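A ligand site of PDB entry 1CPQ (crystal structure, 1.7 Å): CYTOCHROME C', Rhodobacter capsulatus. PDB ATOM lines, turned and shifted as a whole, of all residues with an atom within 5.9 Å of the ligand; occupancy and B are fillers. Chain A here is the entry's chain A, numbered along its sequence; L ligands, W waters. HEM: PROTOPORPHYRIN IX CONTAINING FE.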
ATOM      1  N   LEU A   7       8.503  22.692   4.982  1.00  0.00           N
ATOM      2  CA  LEU A   7       9.651  23.577   5.156  1.00  0.00           C
ATOM      3  C   LEU A   7       9.213  25.038   5.133  1.00  0.00           C
ATOM      4  O   LEU A   7       9.642  25.834   5.962  1.00  0.00           O
ATOM      5  CB  LEU A   7      10.731  23.299   4.097  1.00  0.00           C
ATOM      6  CG  LEU A   7      11.836  22.285   4.497  1.00  0.00           C
ATOM      7  CD1 LEU A   7      11.240  20.975   4.945  1.00  0.00           C
ATOM      8  CD2 LEU A   7      12.763  22.031   3.322  1.00  0.00           C
ATOM      9  N   ARG A  10       7.089  25.770   8.528  1.00  0.00           N
ATOM     10  CA  ARG A  10       7.839  25.925   9.759  1.00  0.00           C
ATOM     11  C   ARG A  10       8.739  27.139   9.737  1.00  0.00           C
ATOM     12  O   ARG A  10       8.960  27.790  10.759  1.00  0.00           O
ATOM     13  CB  ARG A  10       8.593  24.635  10.134  1.00  0.00           C
ATOM     14  CG  ARG A  10       9.692  24.218   9.215  1.00  0.00           C
ATOM     15  CD  ARG A  10      10.056  22.798   9.524  1.00  0.00           C
ATOM     16  NE  ARG A  10      11.383  22.439   9.061  1.00  0.00           N
ATOM     17  CZ  ARG A  10      11.792  21.196   8.838  1.00  0.00           C
ATOM     18  NH1 ARG A  10      10.955  20.183   8.993  1.00  0.00           N
ATOM     19  NH2 ARG A  10      13.032  20.974   8.415  1.00  0.00           N
ATOM     20  N   GLU A  11       9.240  27.493   8.571  1.00  0.00           N
ATOM     21  CA  GLU A  11      10.095  28.661   8.481  1.00  0.00           C
ATOM     22  C   GLU A  11       9.253  29.921   8.676  1.00  0.00           C
ATOM     23  O   GLU A  11       9.675  30.861   9.347  1.00  0.00           O
ATOM     24  CB  GLU A  11      10.898  28.642   7.167  1.00  0.00           C
ATOM     25  CG  GLU A  11      12.102  27.650   7.265  1.00  0.00           C
ATOM     26  CD  GLU A  11      12.587  27.084   5.924  1.00  0.00           C
ATOM     27  OE1 GLU A  11      12.476  27.787   4.887  1.00  0.00           O
ATOM     28  OE2 GLU A  11      13.066  25.927   5.907  1.00  0.00           O
ATOM     29  N   ALA A  12       8.008  29.885   8.215  1.00  0.00           N
ATOM     30  CA  ALA A  12       7.090  30.997   8.359  1.00  0.00           C
ATOM     31  C   ALA A  12       6.731  31.185   9.818  1.00  0.00           C
ATOM     32  O   ALA A  12       6.637  32.309  10.321  1.00  0.00           O
ATOM     33  CB  ALA A  12       5.816  30.726   7.564  1.00  0.00           C
ATOM     34  N   PHE A  14       8.538  30.190  12.539  1.00  0.00           N
ATOM     35  CA  PHE A  14       9.678  30.696  13.303  1.00  0.00           C
ATOM     36  C   PHE A  14       9.987  32.153  12.985  1.00  0.00           C
ATOM     37  O   PHE A  14      10.417  32.918  13.857  1.00  0.00           O
ATOM     38  CB  PHE A  14      10.914  29.808  13.110  1.00  0.00           C
ATOM     39  CG  PHE A  14      10.819  28.500  13.844  1.00  0.00           C
ATOM     40  CD1 PHE A  14      10.654  28.487  15.207  1.00  0.00           C
ATOM     41  CD2 PHE A  14      10.862  27.302  13.157  1.00  0.00           C
ATOM     42  CE1 PHE A  14      10.524  27.283  15.896  1.00  0.00           C
ATOM     43  CE2 PHE A  14      10.732  26.097  13.824  1.00  0.00           C
ATOM     44  CZ  PHE A  14      10.559  26.091  15.200  1.00  0.00           C
ATOM     45  N   LYS A  15       9.748  32.544  11.726  1.00  0.00           N
ATOM     46  CA  LYS A  15       9.935  33.930  11.315  1.00  0.00           C
ATOM     47  C   LYS A  15       8.949  34.814  12.083  1.00  0.00           C
ATOM     48  O   LYS A  15       9.331  35.852  12.612  1.00  0.00           O
ATOM     49  CB  LYS A  15       9.720  34.102   9.806  1.00  0.00           C
ATOM     50  CG  LYS A  15      10.985  33.865   8.989  1.00  0.00           C
ATOM     51  CD  LYS A  15      10.800  34.353   7.577  1.00  0.00           C
ATOM     52  CE  LYS A  15      12.117  34.463   6.816  1.00  0.00           C
ATOM     53  NZ  LYS A  15      12.731  33.136   6.519  1.00  0.00           N
ATOM     54  N   LEU A  17       7.613  34.170  14.953  1.00  0.00           N
ATOM     55  CA  LEU A  17       8.024  34.129  16.348  1.00  0.00           C
ATOM     56  C   LEU A  17       9.175  35.115  16.540  1.00  0.00           C
ATOM     57  O   LEU A  17       9.257  35.822  17.556  1.00  0.00           O
ATOM     58  CB  LEU A  17       8.503  32.723  16.758  1.00  0.00           C
ATOM     59  CG  LEU A  17       7.590  31.670  17.368  1.00  0.00           C
ATOM     60  CD1 LEU A  17       8.462  30.505  17.849  1.00  0.00           C
ATOM     61  CD2 LEU A  17       6.834  32.247  18.550  1.00  0.00           C
ATOM     62  N   GLY A  18      10.100  35.144  15.576  1.00  0.00           N
ATOM     63  CA  GLY A  18      11.218  36.066  15.664  1.00  0.00           C
ATOM     64  C   GLY A  18      10.719  37.502  15.709  1.00  0.00           C
ATOM     65  O   GLY A  18      11.152  38.300  16.548  1.00  0.00           O
ATOM     66  N   MET A  21       9.264  38.280  19.074  1.00  0.00           N
ATOM     67  CA  MET A  21      10.296  38.470  20.094  1.00  0.00           C
ATOM     68  C   MET A  21      10.936  39.856  19.969  1.00  0.00           C
ATOM     69  O   MET A  21      11.172  40.546  20.962  1.00  0.00           O
ATOM     70  CB  MET A  21      11.381  37.391  19.942  1.00  0.00           C
ATOM     71  CG  MET A  21      12.345  37.311  21.087  1.00  0.00           C
ATOM     72  SD  MET A  21      11.528  36.779  22.595  1.00  0.00           S
ATOM     73  CE  MET A  21      12.642  37.401  23.806  1.00  0.00           C
ATOM     74  N   PHE A  55       7.601  18.701  11.382  1.00  0.00           N
ATOM     75  CA  PHE A  55       8.918  18.084  11.513  1.00  0.00           C
ATOM     76  C   PHE A  55       8.922  16.573  11.243  1.00  0.00           C
ATOM     77  O   PHE A  55       9.331  15.782  12.106  1.00  0.00           O
ATOM     78  CB  PHE A  55       9.508  18.368  12.887  1.00  0.00           C
ATOM     79  CG  PHE A  55      10.060  19.758  13.040  1.00  0.00           C
ATOM     80  CD1 PHE A  55      11.384  20.031  12.711  1.00  0.00           C
ATOM     81  CD2 PHE A  55       9.270  20.798  13.495  1.00  0.00           C
ATOM     82  CE1 PHE A  55      11.905  21.305  12.830  1.00  0.00           C
ATOM     83  CE2 PHE A  55       9.778  22.089  13.627  1.00  0.00           C
ATOM     84  CZ  PHE A  55      11.098  22.338  13.294  1.00  0.00           C
ATOM     85  N   GLN A  67      18.489  24.002   2.392  1.00  0.00           N
ATOM     86  CA  GLN A  67      17.078  24.380   2.345  1.00  0.00           C
ATOM     87  C   GLN A  67      16.409  24.453   3.718  1.00  0.00           C
ATOM     88  O   GLN A  67      15.253  24.868   3.837  1.00  0.00           O
ATOM     89  CB  GLN A  67      16.323  23.429   1.413  1.00  0.00           C
ATOM     90  CG  GLN A  67      17.001  23.295   0.074  1.00  0.00           C
ATOM     91  CD  GLN A  67      16.039  22.968  -1.057  1.00  0.00           C
ATOM     92  OE1 GLN A  67      16.357  22.166  -1.930  1.00  0.00           O
ATOM     93  NE2 GLN A  67      14.890  23.625  -1.061  1.00  0.00           N
ATOM     94  N   THR A  68      17.157  24.069   4.748  1.00  0.00           N
ATOM     95  CA  THR A  68      16.644  24.093   6.118  1.00  0.00           C
ATOM     96  C   THR A  68      17.814  24.103   7.108  1.00  0.00           C
ATOM     97  O   THR A  68      18.935  23.697   6.788  1.00  0.00           O
ATOM     98  CB  THR A  68      15.706  22.872   6.408  1.00  0.00           C
ATOM     99  OG1 THR A  68      15.332  22.873   7.786  1.00  0.00           O
ATOM    100  CG2 THR A  68      16.400  21.549   6.083  1.00  0.00           C
ATOM    101  N   GLU A  69      17.541  24.618   8.306  1.00  0.00           N
ATOM    102  CA  GLU A  69      18.527  24.677   9.360  1.00  0.00           C
ATOM    103  C   GLU A  69      18.202  23.675  10.463  1.00  0.00           C
ATOM    104  O   GLU A  69      18.788  23.725  11.547  1.00  0.00           O
ATOM    105  CB  GLU A  69      18.602  26.071   9.952  1.00  0.00           C
ATOM    106  CG  GLU A  69      18.980  27.137   8.966  1.00  0.00           C
ATOM    107  CD  GLU A  69      19.290  28.434   9.654  1.00  0.00           C
ATOM    108  OE1 GLU A  69      18.410  29.000  10.341  1.00  0.00           O
ATOM    109  OE2 GLU A  69      20.445  28.902   9.524  1.00  0.00           O
ATOM    110  N   ALA A  70      17.270  22.766  10.194  1.00  0.00           N
ATOM    111  CA  ALA A  70      16.908  21.752  11.181  1.00  0.00           C
ATOM    112  C   ALA A  70      17.950  20.616  11.212  1.00  0.00           C
ATOM    113  O   ALA A  70      18.174  19.953  10.200  1.00  0.00           O
ATOM    114  CB  ALA A  70      15.541  21.191  10.879  1.00  0.00           C
ATOM    115  N   LYS A  71      18.621  20.455  12.345  1.00  0.00           N
ATOM    116  CA  LYS A  71      19.631  19.409  12.515  1.00  0.00           C
ATOM    117  C   LYS A  71      19.041  17.988  12.591  1.00  0.00           C
ATOM    118  O   LYS A  71      17.972  17.776  13.148  1.00  0.00           O
ATOM    119  CB  LYS A  71      20.417  19.648  13.786  1.00  0.00           C
ATOM    120  CG  LYS A  71      21.383  20.781  13.732  1.00  0.00           C
ATOM    121  CD  LYS A  71      22.156  20.805  15.030  1.00  0.00           C
ATOM    122  CE  LYS A  71      23.500  21.402  14.834  1.00  0.00           C
ATOM    123  NZ  LYS A  71      24.356  20.895  15.936  1.00  0.00           N
ATOM    124  N   ILE A  74      17.391  16.405  15.783  1.00  0.00           N
ATOM    125  CA  ILE A  74      15.985  16.537  16.171  1.00  0.00           C
ATOM    126  C   ILE A  74      15.262  15.196  16.187  1.00  0.00           C
ATOM    127  O   ILE A  74      14.534  14.859  17.127  1.00  0.00           O
ATOM    128  CB  ILE A  74      15.233  17.519  15.227  1.00  0.00           C
ATOM    129  CG1 ILE A  74      15.749  18.949  15.455  1.00  0.00           C
ATOM    130  CG2 ILE A  74      13.722  17.428  15.416  1.00  0.00           C
ATOM    131  CD1 ILE A  74      15.278  19.993  14.443  1.00  0.00           C
ATOM    132  N   PHE A  81      13.357  17.240  22.035  1.00  0.00           N
ATOM    133  CA  PHE A  81      12.939  18.313  21.137  1.00  0.00           C
ATOM    134  C   PHE A  81      11.535  18.789  21.538  1.00  0.00           C
ATOM    135  O   PHE A  81      11.273  20.004  21.586  1.00  0.00           O
ATOM    136  CB  PHE A  81      12.943  17.839  19.681  1.00  0.00           C
ATOM    137  CG  PHE A  81      12.602  18.923  18.710  1.00  0.00           C
ATOM    138  CD1 PHE A  81      13.507  19.941  18.442  1.00  0.00           C
ATOM    139  CD2 PHE A  81      11.358  18.936  18.077  1.00  0.00           C
ATOM    140  CE1 PHE A  81      13.185  20.949  17.551  1.00  0.00           C
ATOM    141  CE2 PHE A  81      11.036  19.943  17.186  1.00  0.00           C
ATOM    142  CZ  PHE A  81      11.953  20.957  16.914  1.00  0.00           C
ATOM    143  N   GLY A  82      10.667  17.845  21.860  1.00  0.00           N
ATOM    144  CA  GLY A  82       9.319  18.193  22.279  1.00  0.00           C
ATOM    145  C   GLY A  82       9.302  18.879  23.642  1.00  0.00           C
ATOM    146  O   GLY A  82       8.499  19.783  23.888  1.00  0.00           O
ATOM    147  N   LYS A  84      11.695  20.783  24.897  1.00  0.00           N
ATOM    148  CA  LYS A  84      12.175  22.147  24.694  1.00  0.00           C
ATOM    149  C   LYS A  84      11.061  23.030  24.116  1.00  0.00           C
ATOM    150  O   LYS A  84      10.985  24.232  24.431  1.00  0.00           O
ATOM    151  CB  LYS A  84      13.394  22.138  23.760  1.00  0.00           C
ATOM    152  CG  LYS A  84      14.588  21.323  24.249  1.00  0.00           C
ATOM    153  CD  LYS A  84      15.726  22.202  24.679  1.00  0.00           C
ATOM    154  CE  LYS A  84      17.039  21.420  24.888  1.00  0.00           C
ATOM    155  NZ  LYS A  84      17.004  20.477  26.044  1.00  0.00           N
ATOM    156  N   GLY A  85      10.212  22.446  23.281  1.00  0.00           N
ATOM    157  CA  GLY A  85       9.101  23.176  22.718  1.00  0.00           C
ATOM    158  C   GLY A  85       8.066  23.486  23.794  1.00  0.00           C
ATOM    159  O   GLY A  85       7.495  24.579  23.814  1.00  0.00           O
ATOM    160  N   MET A  88       9.085  26.449  25.875  1.00  0.00           N
ATOM    161  CA  MET A  88       8.797  27.737  25.258  1.00  0.00           C
ATOM    162  C   MET A  88       7.332  28.121  25.439  1.00  0.00           C
ATOM    163  O   MET A  88       7.028  29.262  25.764  1.00  0.00           O
ATOM    164  CB  MET A  88       9.141  27.729  23.760  1.00  0.00           C
ATOM    165  CG  MET A  88       8.718  29.017  23.059  1.00  0.00           C
ATOM    166  SD  MET A  88       8.856  28.968  21.282  1.00  0.00           S
ATOM    167  CE  MET A  88       7.384  28.046  20.907  1.00  0.00           C
ATOM    168  N   LEU A 114      11.469  33.506  28.267  1.00  0.00           N
ATOM    169  CA  LEU A 114      11.070  33.079  26.919  1.00  0.00           C
ATOM    170  C   LEU A 114      12.297  33.086  26.012  1.00  0.00           C
ATOM    171  O   LEU A 114      12.558  32.100  25.349  1.00  0.00           O
ATOM    172  CB  LEU A 114       9.976  33.994  26.358  1.00  0.00           C
ATOM    173  CG  LEU A 114       9.440  33.645  24.963  1.00  0.00           C
ATOM    174  CD1 LEU A 114       8.890  32.217  24.932  1.00  0.00           C
ATOM    175  CD2 LEU A 114       8.367  34.641  24.541  1.00  0.00           C
ATOM    176  N   GLY A 115      13.090  34.153  26.056  1.00  0.00           N
ATOM    177  CA  GLY A 115      14.301  34.223  25.254  1.00  0.00           C
ATOM    178  C   GLY A 115      15.204  33.031  25.511  1.00  0.00           C
ATOM    179  O   GLY A 115      15.783  32.459  24.582  1.00  0.00           O
ATOM    180  N   THR A 117      14.400  30.026  26.290  1.00  0.00           N
ATOM    181  CA  THR A 117      13.881  28.810  25.668  1.00  0.00           C
ATOM    182  C   THR A 117      14.189  28.774  24.171  1.00  0.00           C
ATOM    183  O   THR A 117      14.354  27.681  23.604  1.00  0.00           O
ATOM    184  CB  THR A 117      12.384  28.618  25.910  1.00  0.00           C
ATOM    185  OG1 THR A 117      11.651  29.607  25.194  1.00  0.00           O
ATOM    186  CG2 THR A 117      12.051  28.709  27.404  1.00  0.00           C
ATOM    187  N   CYS A 118      14.287  29.931  23.520  1.00  0.00           N
ATOM    188  CA  CYS A 118      14.635  29.983  22.095  1.00  0.00           C
ATOM    189  C   CYS A 118      16.062  29.474  21.987  1.00  0.00           C
ATOM    190  O   CYS A 118      16.369  28.592  21.185  1.00  0.00           O
ATOM    191  CB  CYS A 118      14.636  31.408  21.545  1.00  0.00           C
ATOM    192  SG  CYS A 118      13.224  32.454  21.939  1.00  0.00           S
ATOM    193  N   LYS A 119      16.948  30.041  22.809  1.00  0.00           N
ATOM    194  CA  LYS A 119      18.363  29.673  22.806  1.00  0.00           C
ATOM    195  C   LYS A 119      18.592  28.215  23.154  1.00  0.00           C
ATOM    196  O   LYS A 119      19.343  27.533  22.456  1.00  0.00           O
ATOM    197  CB  LYS A 119      19.176  30.564  23.749  1.00  0.00           C
ATOM    198  CG  LYS A 119      20.627  30.172  23.792  1.00  0.00           C
ATOM    199  CD  LYS A 119      21.408  31.026  24.759  1.00  0.00           C
ATOM    200  CE  LYS A 119      22.788  30.420  25.005  1.00  0.00           C
ATOM    201  NZ  LYS A 119      23.555  30.154  23.738  1.00  0.00           N
ATOM    202  N   CYS A 121      16.814  25.600  22.667  1.00  0.00           N
ATOM    203  CA  CYS A 121      16.522  24.714  21.558  1.00  0.00           C
ATOM    204  C   CYS A 121      17.478  24.960  20.388  1.00  0.00           C
ATOM    205  O   CYS A 121      17.963  24.003  19.771  1.00  0.00           O
ATOM    206  CB  CYS A 121      15.085  24.865  21.082  1.00  0.00           C
ATOM    207  SG  CYS A 121      14.723  23.631  19.801  1.00  0.00           S
ATOM    208  N   HIS A 122      17.745  26.221  20.084  1.00  0.00           N
ATOM    209  CA  HIS A 122      18.631  26.547  18.982  1.00  0.00           C
ATOM    210  C   HIS A 122      20.018  25.930  19.126  1.00  0.00           C
ATOM    211  O   HIS A 122      20.563  25.373  18.151  1.00  0.00           O
ATOM    212  CB  HIS A 122      18.729  28.066  18.817  1.00  0.00           C
ATOM    213  CG  HIS A 122      17.493  28.681  18.229  1.00  0.00           C
ATOM    214  ND1 HIS A 122      17.263  30.039  18.146  1.00  0.00           N
ATOM    215  CD2 HIS A 122      16.394  28.092  17.684  1.00  0.00           C
ATOM    216  CE1 HIS A 122      16.066  30.220  17.572  1.00  0.00           C
ATOM    217  NE2 HIS A 122      15.501  29.062  17.274  1.00  0.00           N
ATOM    218  N   TYR A 125      19.538  22.031  18.315  1.00  0.00           N
ATOM    219  CA  TYR A 125      18.829  21.631  17.095  1.00  0.00           C
ATOM    220  C   TYR A 125      18.811  22.513  15.866  1.00  0.00           C
ATOM    221  O   TYR A 125      18.202  22.146  14.863  1.00  0.00           O
ATOM    222  CB  TYR A 125      17.380  21.280  17.491  1.00  0.00           C
ATOM    223  CG  TYR A 125      17.318  20.256  18.602  1.00  0.00           C
ATOM    224  CD1 TYR A 125      17.801  18.961  18.403  1.00  0.00           C
ATOM    225  CD2 TYR A 125      16.840  20.602  19.872  1.00  0.00           C
ATOM    226  CE1 TYR A 125      17.805  18.031  19.424  1.00  0.00           C
ATOM    227  CE2 TYR A 125      16.836  19.669  20.920  1.00  0.00           C
ATOM    228  CZ  TYR A 125      17.331  18.389  20.688  1.00  0.00           C
ATOM    229  OH  TYR A 125      17.368  17.452  21.696  1.00  0.00           O
ATOM    230  N   ARG A 126      19.447  23.673  15.926  1.00  0.00           N
ATOM    231  CA  ARG A 126      19.459  24.561  14.772  1.00  0.00           C
ATOM    232  C   ARG A 126      20.888  24.766  14.275  1.00  0.00           C
ATOM    233  O   ARG A 126      21.791  24.998  15.084  1.00  0.00           O
ATOM    234  CB  ARG A 126      18.846  25.912  15.131  1.00  0.00           C
ATOM    235  CG  ARG A 126      18.660  26.840  13.969  1.00  0.00           C
ATOM    236  CD  ARG A 126      18.216  28.186  14.443  1.00  0.00           C
ATOM    237  NE  ARG A 126      18.154  29.141  13.341  1.00  0.00           N
ATOM    238  CZ  ARG A 126      17.911  30.436  13.484  1.00  0.00           C
ATOM    239  NH1 ARG A 126      17.699  30.958  14.686  1.00  0.00           N
ATOM    240  NH2 ARG A 126      17.904  31.219  12.412  1.00  0.00           N
HETATM  241  CHA HEM L   1      14.557  28.511  13.287  1.00  0.00           C
HETATM  242  CHB HEM L   1      13.197  32.152  16.186  1.00  0.00           C
HETATM  243  CHC HEM L   1      12.305  28.977  19.637  1.00  0.00           C
HETATM  244  CHD HEM L   1      13.711  25.316  16.801  1.00  0.00           C
HETATM  245  C1A HEM L   1      14.261  29.783  13.768  1.00  0.00           C
HETATM  246  C2A HEM L   1      14.374  30.985  12.962  1.00  0.00           C
HETATM  247  C3A HEM L   1      13.991  32.031  13.780  1.00  0.00           C
HETATM  248  C4A HEM L   1      13.617  31.421  15.077  1.00  0.00           C
HETATM  249  CMA HEM L   1      13.981  33.537  13.464  1.00  0.00           C
HETATM  250  CAA HEM L   1      14.782  31.063  11.491  1.00  0.00           C
HETATM  251  CBA HEM L   1      13.522  30.929  10.676  1.00  0.00           C
HETATM  252  CGA HEM L   1      13.687  31.392   9.231  1.00  0.00           C
HETATM  253  O1A HEM L   1      13.846  32.617   9.011  1.00  0.00           O
HETATM  254  O2A HEM L   1      13.630  30.545   8.319  1.00  0.00           O
HETATM  255  C1B HEM L   1      12.859  31.588  17.387  1.00  0.00           C
HETATM  256  C2B HEM L   1      12.431  32.350  18.549  1.00  0.00           C
HETATM  257  C3B HEM L   1      12.206  31.411  19.532  1.00  0.00           C
HETATM  258  C4B HEM L   1      12.464  30.140  18.945  1.00  0.00           C
HETATM  259  CMB HEM L   1      12.311  33.879  18.698  1.00  0.00           C
HETATM  260  CAB HEM L   1      11.874  31.679  21.014  1.00  0.00           C
HETATM  261  CBB HEM L   1      10.527  32.351  21.235  1.00  0.00           C
HETATM  262  C1C HEM L   1      12.609  27.710  19.174  1.00  0.00           C
HETATM  263  C2C HEM L   1      12.346  26.482  19.978  1.00  0.00           C
HETATM  264  C3C HEM L   1      12.753  25.458  19.154  1.00  0.00           C
HETATM  265  C4C HEM L   1      13.234  26.053  17.902  1.00  0.00           C
HETATM  266  CMC HEM L   1      11.823  26.449  21.435  1.00  0.00           C
HETATM  267  CAC HEM L   1      12.974  23.993  19.440  1.00  0.00           C
HETATM  268  CBC HEM L   1      11.937  23.326  20.383  1.00  0.00           C
HETATM  269  C1D HEM L   1      14.054  25.871  15.601  1.00  0.00           C
HETATM  270  C2D HEM L   1      14.519  25.093  14.448  1.00  0.00           C
HETATM  271  C3D HEM L   1      14.765  25.987  13.467  1.00  0.00           C
HETATM  272  C4D HEM L   1      14.436  27.311  13.994  1.00  0.00           C
HETATM  273  CMD HEM L   1      14.635  23.564  14.334  1.00  0.00           C
HETATM  274  CAD HEM L   1      15.131  25.594  12.034  1.00  0.00           C
HETATM  275  CBD HEM L   1      13.875  25.450  11.175  1.00  0.00           C
HETATM  276  CGD HEM L   1      14.198  25.201   9.715  1.00  0.00           C
HETATM  277  O1D HEM L   1      15.231  25.708   9.235  1.00  0.00           O
HETATM  278  O2D HEM L   1      13.426  24.505   9.032  1.00  0.00           O
HETATM  279  NA  HEM L   1      13.801  30.049  15.072  1.00  0.00           N
HETATM  280  NB  HEM L   1      12.907  30.229  17.647  1.00  0.00           N
HETATM  281  NC  HEM L   1      13.139  27.434  17.919  1.00  0.00           N
HETATM  282  ND  HEM L   1      14.026  27.238  15.318  1.00  0.00           N
HETATM  283 FE   HEM L   1      13.656  28.758  16.540  1.00  0.00          FE
HETATM  284  O   HOH W   1      14.378  35.666  10.346  1.00  0.00           O
HETATM  285  O   HOH W   2      15.797  28.539   9.657  1.00  0.00           O
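The side-chain sulfur (SG) of Cys 118 is bonded to a carbon (CAB) of the ligand (1.8 Å). The side-chain sulfur (SG) of Cys 121 is covalently linked to a carbon (CAC) of the ligand. A ring nitrogen (NE2) of His 122 is bound to an iron atom (FE) of the ligand, at 2.0 Å. The backbone NH (N) of Glu 69 sits at hydrogen-bond distance from an oxygen (O1D) of the ligand (2.7 Å). NZ of Lys 15 lies within salt-bridge range of O1A of the ligand (2.8 Å). O2D of the ligand lies within hydrogen-bond range of OG1 of Thr 68, at 2.8 Å. The guanidinium group of Arg 10 is in salt-bridge range of an oxygen (O2D) of the ligand (2.9 Å).
The backbone carbonyl oxygen of Cys 118 sits close to a ring nitrogen (ND1) of His 122 (3.5 Å). The guanidinium group (NE) of Arg 126 lies within salt-bridge range of the side-chain carboxylate (OE1) of Glu 69, 3.0 Å away. OG1 of Thr 68 lies within hydrogen-bond range of NH2 of Arg 10, at 3.0 Å. The backbone NH of Ala 70 lies within hydrogen-bond range of the side-chain hydroxyl of Thr 68. The backbone carbonyl oxygen of Leu 114 sits at hydrogen-bond distance from the side-chain hydroxyl of Thr 117. The backbone carbonyl oxygen of Tyr 125 is in hydrogen-bond range of the backbone NH of Lys 71, 3.1 Å away.
The side-chain carboxylate (OE2) of Glu 11 sits close to an oxygen (O2D) of the ligand (3.5 Å). Residues that only touch the ligand: Phe 14 (3.3 Å), Leu 17 (3.8 Å), Gly 18 (3.9 Å), Met 21 (3.8 Å), Phe 55 (3.8 Å), Ala 70 (3.7 Å), Ile 74 (3.6 Å), Phe 81 (3.6 Å), Lys 84 (3.8 Å), Gly 85 (3.5 Å), Met 88 (3.8 Å), Thr 117 (3.6 Å), Tyr 125 (3.9 Å) and Arg 126 (3.3 Å). Within 4 Å of the ligand: Arg 10, Glu 11, Phe 14, Lys 15, Leu 17, Gly 18, Met 21, Phe 55, Thr 68, Glu 69, Ala 70, Ile 74, Phe 81, Lys 84, Gly 85, Met 88, Thr 117, Cys 118, Cys 121, His 122, Tyr 125 and Arg 126.
Water W2 lies within hydrogen-bond range of OE1 of Glu 69 (2.7 Å) and O1D of the ligand (2.9 Å).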
